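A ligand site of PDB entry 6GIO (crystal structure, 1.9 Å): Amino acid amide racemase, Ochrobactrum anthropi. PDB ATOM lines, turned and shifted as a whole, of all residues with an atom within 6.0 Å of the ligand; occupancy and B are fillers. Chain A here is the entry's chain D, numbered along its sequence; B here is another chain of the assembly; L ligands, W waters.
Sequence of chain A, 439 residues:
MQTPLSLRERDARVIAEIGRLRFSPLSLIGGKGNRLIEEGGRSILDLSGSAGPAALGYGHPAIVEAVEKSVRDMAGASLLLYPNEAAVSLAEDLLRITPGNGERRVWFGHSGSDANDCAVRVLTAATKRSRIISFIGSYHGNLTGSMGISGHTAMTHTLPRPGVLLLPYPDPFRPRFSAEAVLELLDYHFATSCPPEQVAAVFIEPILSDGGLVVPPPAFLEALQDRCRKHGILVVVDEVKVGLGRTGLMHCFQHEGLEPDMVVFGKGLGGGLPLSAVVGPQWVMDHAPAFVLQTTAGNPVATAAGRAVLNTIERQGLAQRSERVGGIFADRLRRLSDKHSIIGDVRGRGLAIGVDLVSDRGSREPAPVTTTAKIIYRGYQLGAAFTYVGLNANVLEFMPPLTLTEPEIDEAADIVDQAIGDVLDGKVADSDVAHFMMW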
ATOM      1  N   ALA A  51      25.383  14.186   9.632  1.00  0.00           N
ATOM      2  CA  ALA A  51      24.809  13.359  10.752  1.00  0.00           C
ATOM      3  C   ALA A  51      24.310  11.965  10.429  1.00  0.00           C
ATOM      4  O   ALA A  51      23.688  11.338  11.275  1.00  0.00           O
ATOM      5  CB  ALA A  51      23.751  14.101  11.546  1.00  0.00           C
ATOM      6  N   HIS A 110       9.306  10.281   6.283  1.00  0.00           N
ATOM      7  CA  HIS A 110      10.341  11.230   5.891  1.00  0.00           C
ATOM      8  C   HIS A 110      11.564  11.273   6.804  1.00  0.00           C
ATOM      9  O   HIS A 110      12.649  11.748   6.379  1.00  0.00           O
ATOM     10  CB  HIS A 110       9.734  12.637   5.791  1.00  0.00           C
ATOM     11  CG  HIS A 110       8.574  12.721   4.854  1.00  0.00           C
ATOM     12  ND1 HIS A 110       8.659  12.294   3.538  1.00  0.00           N
ATOM     13  CD2 HIS A 110       7.303  13.142   5.041  1.00  0.00           C
ATOM     14  CE1 HIS A 110       7.483  12.460   2.967  1.00  0.00           C
ATOM     15  NE2 HIS A 110       6.647  12.987   3.839  1.00  0.00           N
ATOM     16  N   SER A 111      11.433  10.861   8.075  1.00  0.00           N
ATOM     17  CA  SER A 111      12.482  11.151   9.022  1.00  0.00           C
ATOM     18  C   SER A 111      12.481  10.131  10.148  1.00  0.00           C
ATOM     19  O   SER A 111      11.518   9.412  10.317  1.00  0.00           O
ATOM     20  CB  SER A 111      12.289  12.579   9.588  1.00  0.00           C
ATOM     21  OG  SER A 111      11.061  12.725  10.306  1.00  0.00           O
ATOM     22  N   GLY A 112      13.570  10.085  10.920  1.00  0.00           N
ATOM     23  CA  GLY A 112      13.583   9.283  12.115  1.00  0.00           C
ATOM     24  C   GLY A 112      12.493   9.728  13.078  1.00  0.00           C
ATOM     25  O   GLY A 112      11.809   8.885  13.700  1.00  0.00           O
ATOM     26  N   SER A 113      12.293  11.044  13.193  1.00  0.00           N
ATOM     27  CA  SER A 113      11.273  11.553  14.077  1.00  0.00           C
ATOM     28  C   SER A 113       9.876  11.029  13.729  1.00  0.00           C
ATOM     29  O   SER A 113       9.115  10.649  14.621  1.00  0.00           O
ATOM     30  CB  SER A 113      11.218  13.081  14.073  1.00  0.00           C
ATOM     31  OG  SER A 113      12.398  13.588  14.620  1.00  0.00           O
ATOM     32  N   ASP A 114       9.487  11.113  12.467  1.00  0.00           N
ATOM     33  CA  ASP A 114       8.124  10.693  12.129  1.00  0.00           C
ATOM     34  C   ASP A 114       7.988   9.135  12.189  1.00  0.00           C
ATOM     35  O   ASP A 114       6.881   8.591  12.476  1.00  0.00           O
ATOM     36  CB  ASP A 114       7.573  11.393  10.830  1.00  0.00           C
ATOM     37  CG  ASP A 114       8.170  10.885   9.500  1.00  0.00           C
ATOM     38  OD1 ASP A 114       8.790   9.806   9.430  1.00  0.00           O
ATOM     39  OD2 ASP A 114       7.982  11.581   8.471  1.00  0.00           O
ATOM     40  N   ASN A 116       9.494   7.056  14.350  1.00  0.00           N
ATOM     41  CA  ASN A 116       9.306   6.732  15.762  1.00  0.00           C
ATOM     42  C   ASN A 116       7.955   7.208  16.279  1.00  0.00           C
ATOM     43  O   ASN A 116       7.398   6.544  17.132  1.00  0.00           O
ATOM     44  CB  ASN A 116      10.406   7.322  16.628  1.00  0.00           C
ATOM     45  CG  ASN A 116      11.628   6.478  16.605  1.00  0.00           C
ATOM     46  OD1 ASN A 116      12.738   7.002  16.493  1.00  0.00           O
ATOM     47  ND2 ASN A 116      11.419   5.134  16.533  1.00  0.00           N
ATOM     48  N   TYR A 139      17.609   9.256  22.056  1.00  0.00           N
ATOM     49  CA  TYR A 139      17.120  10.313  21.170  1.00  0.00           C
ATOM     50  C   TYR A 139      16.339   9.597  20.086  1.00  0.00           C
ATOM     51  O   TYR A 139      16.932   8.956  19.217  1.00  0.00           O
ATOM     52  CB  TYR A 139      18.289  11.100  20.542  1.00  0.00           C
ATOM     53  CG  TYR A 139      17.849  12.279  19.704  1.00  0.00           C
ATOM     54  CD1 TYR A 139      17.393  12.096  18.405  1.00  0.00           C
ATOM     55  CD2 TYR A 139      17.914  13.574  20.198  1.00  0.00           C
ATOM     56  CE1 TYR A 139      16.975  13.178  17.630  1.00  0.00           C
ATOM     57  CE2 TYR A 139      17.502  14.648  19.441  1.00  0.00           C
ATOM     58  CZ  TYR A 139      17.035  14.444  18.159  1.00  0.00           C
ATOM     59  OH  TYR A 139      16.607  15.503  17.402  1.00  0.00           O
ATOM     60  N   HIS A 140      15.013   9.648  20.152  1.00  0.00           N
ATOM     61  CA  HIS A 140      14.218   8.997  19.136  1.00  0.00           C
ATOM     62  C   HIS A 140      13.554   9.970  18.173  1.00  0.00           C
ATOM     63  O   HIS A 140      12.892   9.548  17.246  1.00  0.00           O
ATOM     64  CB  HIS A 140      13.196   8.076  19.813  1.00  0.00           C
ATOM     65  CG  HIS A 140      13.819   6.952  20.586  1.00  0.00           C
ATOM     66  ND1 HIS A 140      14.423   5.886  19.951  1.00  0.00           N
ATOM     67  CD2 HIS A 140      13.915   6.715  21.910  1.00  0.00           C
ATOM     68  CE1 HIS A 140      14.914   5.063  20.871  1.00  0.00           C
ATOM     69  NE2 HIS A 140      14.598   5.530  22.069  1.00  0.00           N
ATOM     70  N   GLY A 141      13.716  11.266  18.390  1.00  0.00           N
ATOM     71  CA  GLY A 141      13.158  12.265  17.503  1.00  0.00           C
ATOM     72  C   GLY A 141      12.799  13.581  18.184  1.00  0.00           C
ATOM     73  O   GLY A 141      12.876  13.708  19.434  1.00  0.00           O
ATOM     74  N   ASN A 142      12.412  14.565  17.367  1.00  0.00           N
ATOM     75  CA  ASN A 142      12.081  15.906  17.875  1.00  0.00           C
ATOM     76  C   ASN A 142      10.647  16.390  17.480  1.00  0.00           C
ATOM     77  O   ASN A 142      10.307  17.588  17.618  1.00  0.00           O
ATOM     78  CB  ASN A 142      13.171  16.895  17.446  1.00  0.00           C
ATOM     79  CG  ASN A 142      13.506  17.890  18.539  1.00  0.00           C
ATOM     80  OD1 ASN A 142      13.170  17.688  19.701  1.00  0.00           O
ATOM     81  ND2 ASN A 142      14.169  18.974  18.192  1.00  0.00           N
ATOM     82  N   GLU A 205      18.066   1.898  21.318  1.00  0.00           N
ATOM     83  CA  GLU A 205      19.198   2.207  20.411  1.00  0.00           C
ATOM     84  C   GLU A 205      20.318   1.160  20.703  1.00  0.00           C
ATOM     85  O   GLU A 205      20.733   1.019  21.862  1.00  0.00           O
ATOM     86  CB  GLU A 205      19.774   3.607  20.662  1.00  0.00           C
ATOM     87  CG  GLU A 205      18.816   4.724  20.469  1.00  0.00           C
ATOM     88  CD  GLU A 205      19.483   6.074  20.631  1.00  0.00           C
ATOM     89  OE1 GLU A 205      20.462   6.339  19.932  1.00  0.00           O
ATOM     90  OE2 GLU A 205      19.015   6.880  21.424  1.00  0.00           O
ATOM     91  N   SER A 209      23.324   6.883  20.680  1.00  0.00           N
ATOM     92  CA  SER A 209      23.861   7.951  19.807  1.00  0.00           C
ATOM     93  C   SER A 209      24.150   9.283  20.490  1.00  0.00           C
ATOM     94  O   SER A 209      25.270   9.531  20.943  1.00  0.00           O
ATOM     95  CB  SER A 209      22.896   8.190  18.614  1.00  0.00           C
ATOM     96  OG  SER A 209      21.655   8.807  19.051  1.00  0.00           O
ATOM     97  N   ASP A 210      23.170  10.181  20.518  1.00  0.00           N
ATOM     98  CA  ASP A 210      23.378  11.500  21.063  1.00  0.00           C
ATOM     99  C   ASP A 210      23.717  11.458  22.536  1.00  0.00           C
ATOM    100  O   ASP A 210      24.279  12.420  23.082  1.00  0.00           O
ATOM    101  CB  ASP A 210      22.177  12.419  20.812  1.00  0.00           C
ATOM    102  CG  ASP A 210      22.194  13.009  19.420  1.00  0.00           C
ATOM    103  OD1 ASP A 210      21.669  12.334  18.526  1.00  0.00           O
ATOM    104  OD2 ASP A 210      22.742  14.123  19.220  1.00  0.00           O
ATOM    105  N   ASP A 238      15.850   1.011  17.290  1.00  0.00           N
ATOM    106  CA  ASP A 238      16.014   2.201  16.491  1.00  0.00           C
ATOM    107  C   ASP A 238      17.375   2.118  15.787  1.00  0.00           C
ATOM    108  O   ASP A 238      18.408   2.258  16.420  1.00  0.00           O
ATOM    109  CB  ASP A 238      15.873   3.430  17.399  1.00  0.00           C
ATOM    110  CG  ASP A 238      15.907   4.739  16.654  1.00  0.00           C
ATOM    111  OD1 ASP A 238      16.362   4.798  15.501  1.00  0.00           O
ATOM    112  OD2 ASP A 238      15.491   5.735  17.271  1.00  0.00           O
ATOM    113  N   GLU A 239      17.375   1.894  14.465  1.00  0.00           N
ATOM    114  CA  GLU A 239      18.613   1.771  13.685  1.00  0.00           C
ATOM    115  C   GLU A 239      18.867   3.035  12.863  1.00  0.00           C
ATOM    116  O   GLU A 239      19.670   3.040  11.940  1.00  0.00           O
ATOM    117  CB  GLU A 239      18.493   0.569  12.698  1.00  0.00           C
ATOM    118  CG  GLU A 239      18.546  -0.807  13.359  1.00  0.00           C
ATOM    119  CD  GLU A 239      19.988  -1.346  13.576  1.00  0.00           C
ATOM    120  OE1 GLU A 239      20.893  -1.082  12.742  1.00  0.00           O
ATOM    121  OE2 GLU A 239      20.226  -2.046  14.585  1.00  0.00           O
ATOM    122  N   VAL A 240      18.149   4.095  13.179  1.00  0.00           N
ATOM    123  CA  VAL A 240      18.183   5.321  12.374  1.00  0.00           C
ATOM    124  C   VAL A 240      19.614   5.833  12.244  1.00  0.00           C
ATOM    125  O   VAL A 240      20.030   6.230  11.128  1.00  0.00           O
ATOM    126  CB  VAL A 240      17.292   6.423  12.969  1.00  0.00           C
ATOM    127  CG1 VAL A 240      17.546   7.783  12.316  1.00  0.00           C
ATOM    128  CG2 VAL A 240      15.822   6.010  12.869  1.00  0.00           C
ATOM    129  N   LYS A 241      20.362   5.812  13.335  1.00  0.00           N
ATOM    130  CA  LYS A 241      21.698   6.392  13.350  1.00  0.00           C
ATOM    131  C   LYS A 241      22.793   5.456  12.883  1.00  0.00           C
ATOM    132  O   LYS A 241      23.659   5.856  12.101  1.00  0.00           O
ATOM    133  CB  LYS A 241      22.046   6.924  14.729  1.00  0.00           C
ATOM    134  CG  LYS A 241      23.362   7.666  14.777  1.00  0.00           C
ATOM    135  CD  LYS A 241      23.228   9.107  14.359  1.00  0.00           C
ATOM    136  CE  LYS A 241      24.430   9.873  14.874  1.00  0.00           C
ATOM    137  NZ  LYS A 241      24.585  11.202  14.267  1.00  0.00           N
ATOM    138  N   LYS A 267      17.721   8.443   8.395  1.00  0.00           N
ATOM    139  CA  LYS A 267      18.970   9.091   8.023  1.00  0.00           C
ATOM    140  C   LYS A 267      19.580   8.498   6.731  1.00  0.00           C
ATOM    141  O   LYS A 267      19.077   8.742   5.650  1.00  0.00           O
ATOM    142  CB  LYS A 267      19.930   9.080   9.214  1.00  0.00           C
ATOM    143  CG  LYS A 267      19.614  10.132  10.293  1.00  0.00           C
ATOM    144  CD  LYS A 267      20.578  10.020  11.461  1.00  0.00           C
ATOM    145  CE  LYS A 267      20.459  11.179  12.468  1.00  0.00           C
ATOM    146  NZ  LYS A 267      19.435  10.886  13.494  1.00  0.00           N
ATOM    147  N   LEU B  80      20.041  21.860   9.481  1.00  0.00           N
ATOM    148  CA  LEU B  80      20.359  22.093  10.899  1.00  0.00           C
ATOM    149  C   LEU B  80      21.853  22.129  11.168  1.00  0.00           C
ATOM    150  O   LEU B  80      22.310  22.934  11.983  1.00  0.00           O
ATOM    151  CB  LEU B  80      19.633  21.130  11.830  1.00  0.00           C
ATOM    152  CG  LEU B  80      19.936  19.634  11.793  1.00  0.00           C
ATOM    153  CD1 LEU B  80      21.088  19.269  12.700  1.00  0.00           C
ATOM    154  CD2 LEU B  80      18.726  18.870  12.272  1.00  0.00           C
ATOM    155  N   HIS B 110       9.352  18.337   6.260  1.00  0.00           N
ATOM    156  CA  HIS B 110       9.046  17.412   5.154  1.00  0.00           C
ATOM    157  C   HIS B 110       7.616  17.280   4.807  1.00  0.00           C
ATOM    158  O   HIS B 110       7.313  16.734   3.740  1.00  0.00           O
ATOM    159  CB  HIS B 110       9.488  16.017   5.526  1.00  0.00           C
ATOM    160  CG  HIS B 110      10.899  15.955   5.955  1.00  0.00           C
ATOM    161  ND1 HIS B 110      11.927  16.302   5.114  1.00  0.00           N
ATOM    162  CD2 HIS B 110      11.451  15.576   7.120  1.00  0.00           C
ATOM    163  CE1 HIS B 110      13.072  16.102   5.739  1.00  0.00           C
ATOM    164  NE2 HIS B 110      12.813  15.690   6.964  1.00  0.00           N
ATOM    165  N   LEU B 293      14.007  19.969  15.431  1.00  0.00           N
ATOM    166  CA  LEU B 293      15.055  19.483  14.557  1.00  0.00           C
ATOM    167  C   LEU B 293      14.651  18.239  13.817  1.00  0.00           C
ATOM    168  O   LEU B 293      14.099  17.296  14.416  1.00  0.00           O
ATOM    169  CB  LEU B 293      16.275  19.107  15.377  1.00  0.00           C
ATOM    170  CG  LEU B 293      17.014  20.217  16.144  1.00  0.00           C
ATOM    171  CD1 LEU B 293      18.299  19.616  16.714  1.00  0.00           C
ATOM    172  CD2 LEU B 293      17.308  21.414  15.267  1.00  0.00           C
ATOM    173  N   GLN B 294      14.904  18.221  12.518  1.00  0.00           N
ATOM    174  CA  GLN B 294      14.848  16.974  11.754  1.00  0.00           C
ATOM    175  C   GLN B 294      16.025  16.974  10.820  1.00  0.00           C
ATOM    176  O   GLN B 294      16.172  17.907  10.028  1.00  0.00           O
ATOM    177  CB  GLN B 294      13.578  16.854  10.951  1.00  0.00           C
ATOM    178  CG  GLN B 294      12.348  16.518  11.767  1.00  0.00           C
ATOM    179  CD  GLN B 294      11.123  16.553  10.901  1.00  0.00           C
ATOM    180  OE1 GLN B 294      10.715  17.632  10.445  1.00  0.00           O
ATOM    181  NE2 GLN B 294      10.564  15.382  10.606  1.00  0.00           N
ATOM    182  N   THR B 295      16.809  15.906  10.878  1.00  0.00           N
ATOM    183  CA  THR B 295      18.120  15.881  10.219  1.00  0.00           C
ATOM    184  C   THR B 295      18.162  16.414   8.769  1.00  0.00           C
ATOM    185  O   THR B 295      18.970  17.327   8.455  1.00  0.00           O
ATOM    186  CB  THR B 295      18.751  14.495  10.308  1.00  0.00           C
ATOM    187  OG1 THR B 295      18.926  14.149  11.693  1.00  0.00           O
ATOM    188  CG2 THR B 295      20.138  14.498   9.645  1.00  0.00           C
ATOM    189  N   THR B 296      17.321  15.849   7.901  1.00  0.00           N
ATOM    190  CA  THR B 296      17.352  16.187   6.472  1.00  0.00           C
ATOM    191  C   THR B 296      16.409  17.289   6.047  1.00  0.00           C
ATOM    192  O   THR B 296      16.310  17.576   4.873  1.00  0.00           O
ATOM    193  CB  THR B 296      17.088  14.960   5.572  1.00  0.00           C
ATOM    194  OG1 THR B 296      15.767  14.483   5.805  1.00  0.00           O
ATOM    195  CG2 THR B 296      18.100  13.876   5.853  1.00  0.00           C
HETATM  196  N1  LIG L   1      16.481   8.071  16.220  1.00  0.00           N
HETATM  197  C1  LIG L   1      17.849   8.031  16.259  1.00  0.00           C
HETATM  198  C2  LIG L   1      18.600   6.896  16.924  1.00  0.00           C
HETATM  199  C3  LIG L   1      18.632   9.137  15.625  1.00  0.00           C
HETATM  200  O1  LIG L   1      19.988   9.181  15.626  1.00  0.00           O
HETATM  201  C4  LIG L   1      17.883  10.234  14.966  1.00  0.00           C
HETATM  202  C5  LIG L   1      18.591  11.360  14.311  1.00  0.00           C
HETATM  203  C6  LIG L   1      16.399  10.183  14.998  1.00  0.00           C
HETATM  204  C7  LIG L   1      15.781   9.089  15.624  1.00  0.00           C
HETATM  205  C8  LIG L   1      15.630  11.331  14.323  1.00  0.00           C
HETATM  206  O2  LIG L   1      15.797  11.425  12.886  1.00  0.00           O
HETATM  207  P1  LIG L   1      15.387  12.775  12.125  1.00  0.00           P
HETATM  208  O3  LIG L   1      16.391  13.775  12.689  1.00  0.00           O
HETATM  209  O4  LIG L   1      13.983  13.162  12.575  1.00  0.00           O
HETATM  210  O5  LIG L   1      15.517  12.448  10.675  1.00  0.00           O
HETATM  211  O   HOH W   1      16.408  10.611   9.156  1.00  0.00           O
HETATM  212  O   HOH W   2      15.044  14.147   8.605  1.00  0.00           O
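NZ of Lys 267 is covalently linked to C5 of the ligand (1.3 Å).
An oxygen (O4) of the ligand lies within hydrogen-bond range of the backbone NH (N) of Ser 113, 2.8 Å away.
An oxygen (O4) of the ligand sits at hydrogen-bond distance from the side-chain hydroxyl of Ser 113 (2.6 Å).
The side-chain carboxylate (OD2) of Asp 238 sits at hydrogen-bond distance from a nitrogen (N1) of the ligand, 2.7 Å away.
The backbone NH (N) of Thr 295 of chain B lies within hydrogen-bond range of an oxygen (O3) of the ligand.
OG1 of Thr 295 of chain B lies within hydrogen-bond range of O3 of the ligand (2.7 Å).
An oxygen (O5) of the ligand sits at hydrogen-bond distance from the backbone NH (N) of Gly 112, 3.1 Å away.
The side-chain carboxylate (OD2) of Asp 238 is in hydrogen-bond range of a ring nitrogen (ND1) of His 140 (2.9 Å).
N of Val 240 lies close to OD1 of Asp 238 (3.0 Å).
The side-chain amide oxygen (OD1) of Asn 116 lies close to the backbone carbonyl oxygen (O) of Gly 112 (3.5 Å).
The backbone NH (N) of Tyr 139 sits at hydrogen-bond distance from the side-chain carboxylate (OE2) of Glu 205 (2.8 Å).
The side-chain amino group (NZ) of Lys 241 is in hydrogen-bond range of the backbone carbonyl oxygen (O) of Ala 51 (3.1 Å).
The backbone carbonyl oxygen (O) of His 140 sits close to the side-chain amide oxygen (OD1) of Asn 116, 2.7 Å away.
OG of Ser 111 is in hydrogen-bond range of N of Asp 114 (3.1 Å).
The side-chain carboxylate (OE1) of Glu 205 lies within hydrogen-bond range of the side-chain hydroxyl (OG) of Ser 209.
O of Tyr 139 sits close to N1 of the ligand, 3.2 Å away.
Ser 111 touches the ligand (CB to O5, 3.4 Å).
Asn 116 touches the ligand (OD1 to C7, 3.8 Å).
His 140 touches the ligand (O to C7, 3.3 Å).
Glu 205 touches the ligand.
OG of Ser 209 touches O1 of the ligand, 3.8 Å away.
Val 240 touches the ligand (CG1 to C4, 3.6 Å).
Lys 241 touches the ligand (CB to O1, 3.2 Å).
Gln 294 of chain B touches the ligand.
Hydrophobic or aromatic side chains within 4 Å of the ligand: Tyr 139 and Val 240.
Water W1 lies within hydrogen-bond range of O5 of the ligand (2.5 Å), N of Lys 267 (2.6 Å) and N of Gly 112 (3.4 Å).
Water W2 lies within hydrogen-bond range of an oxygen (O5) of the ligand (2.7 Å), the side-chain hydroxyl of Thr 296 of chain B (2.9 Å), a ring nitrogen (NE2) of His 110 of chain B (3.2 Å) and the backbone NH of Thr 295 of chain B (3.4 Å).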
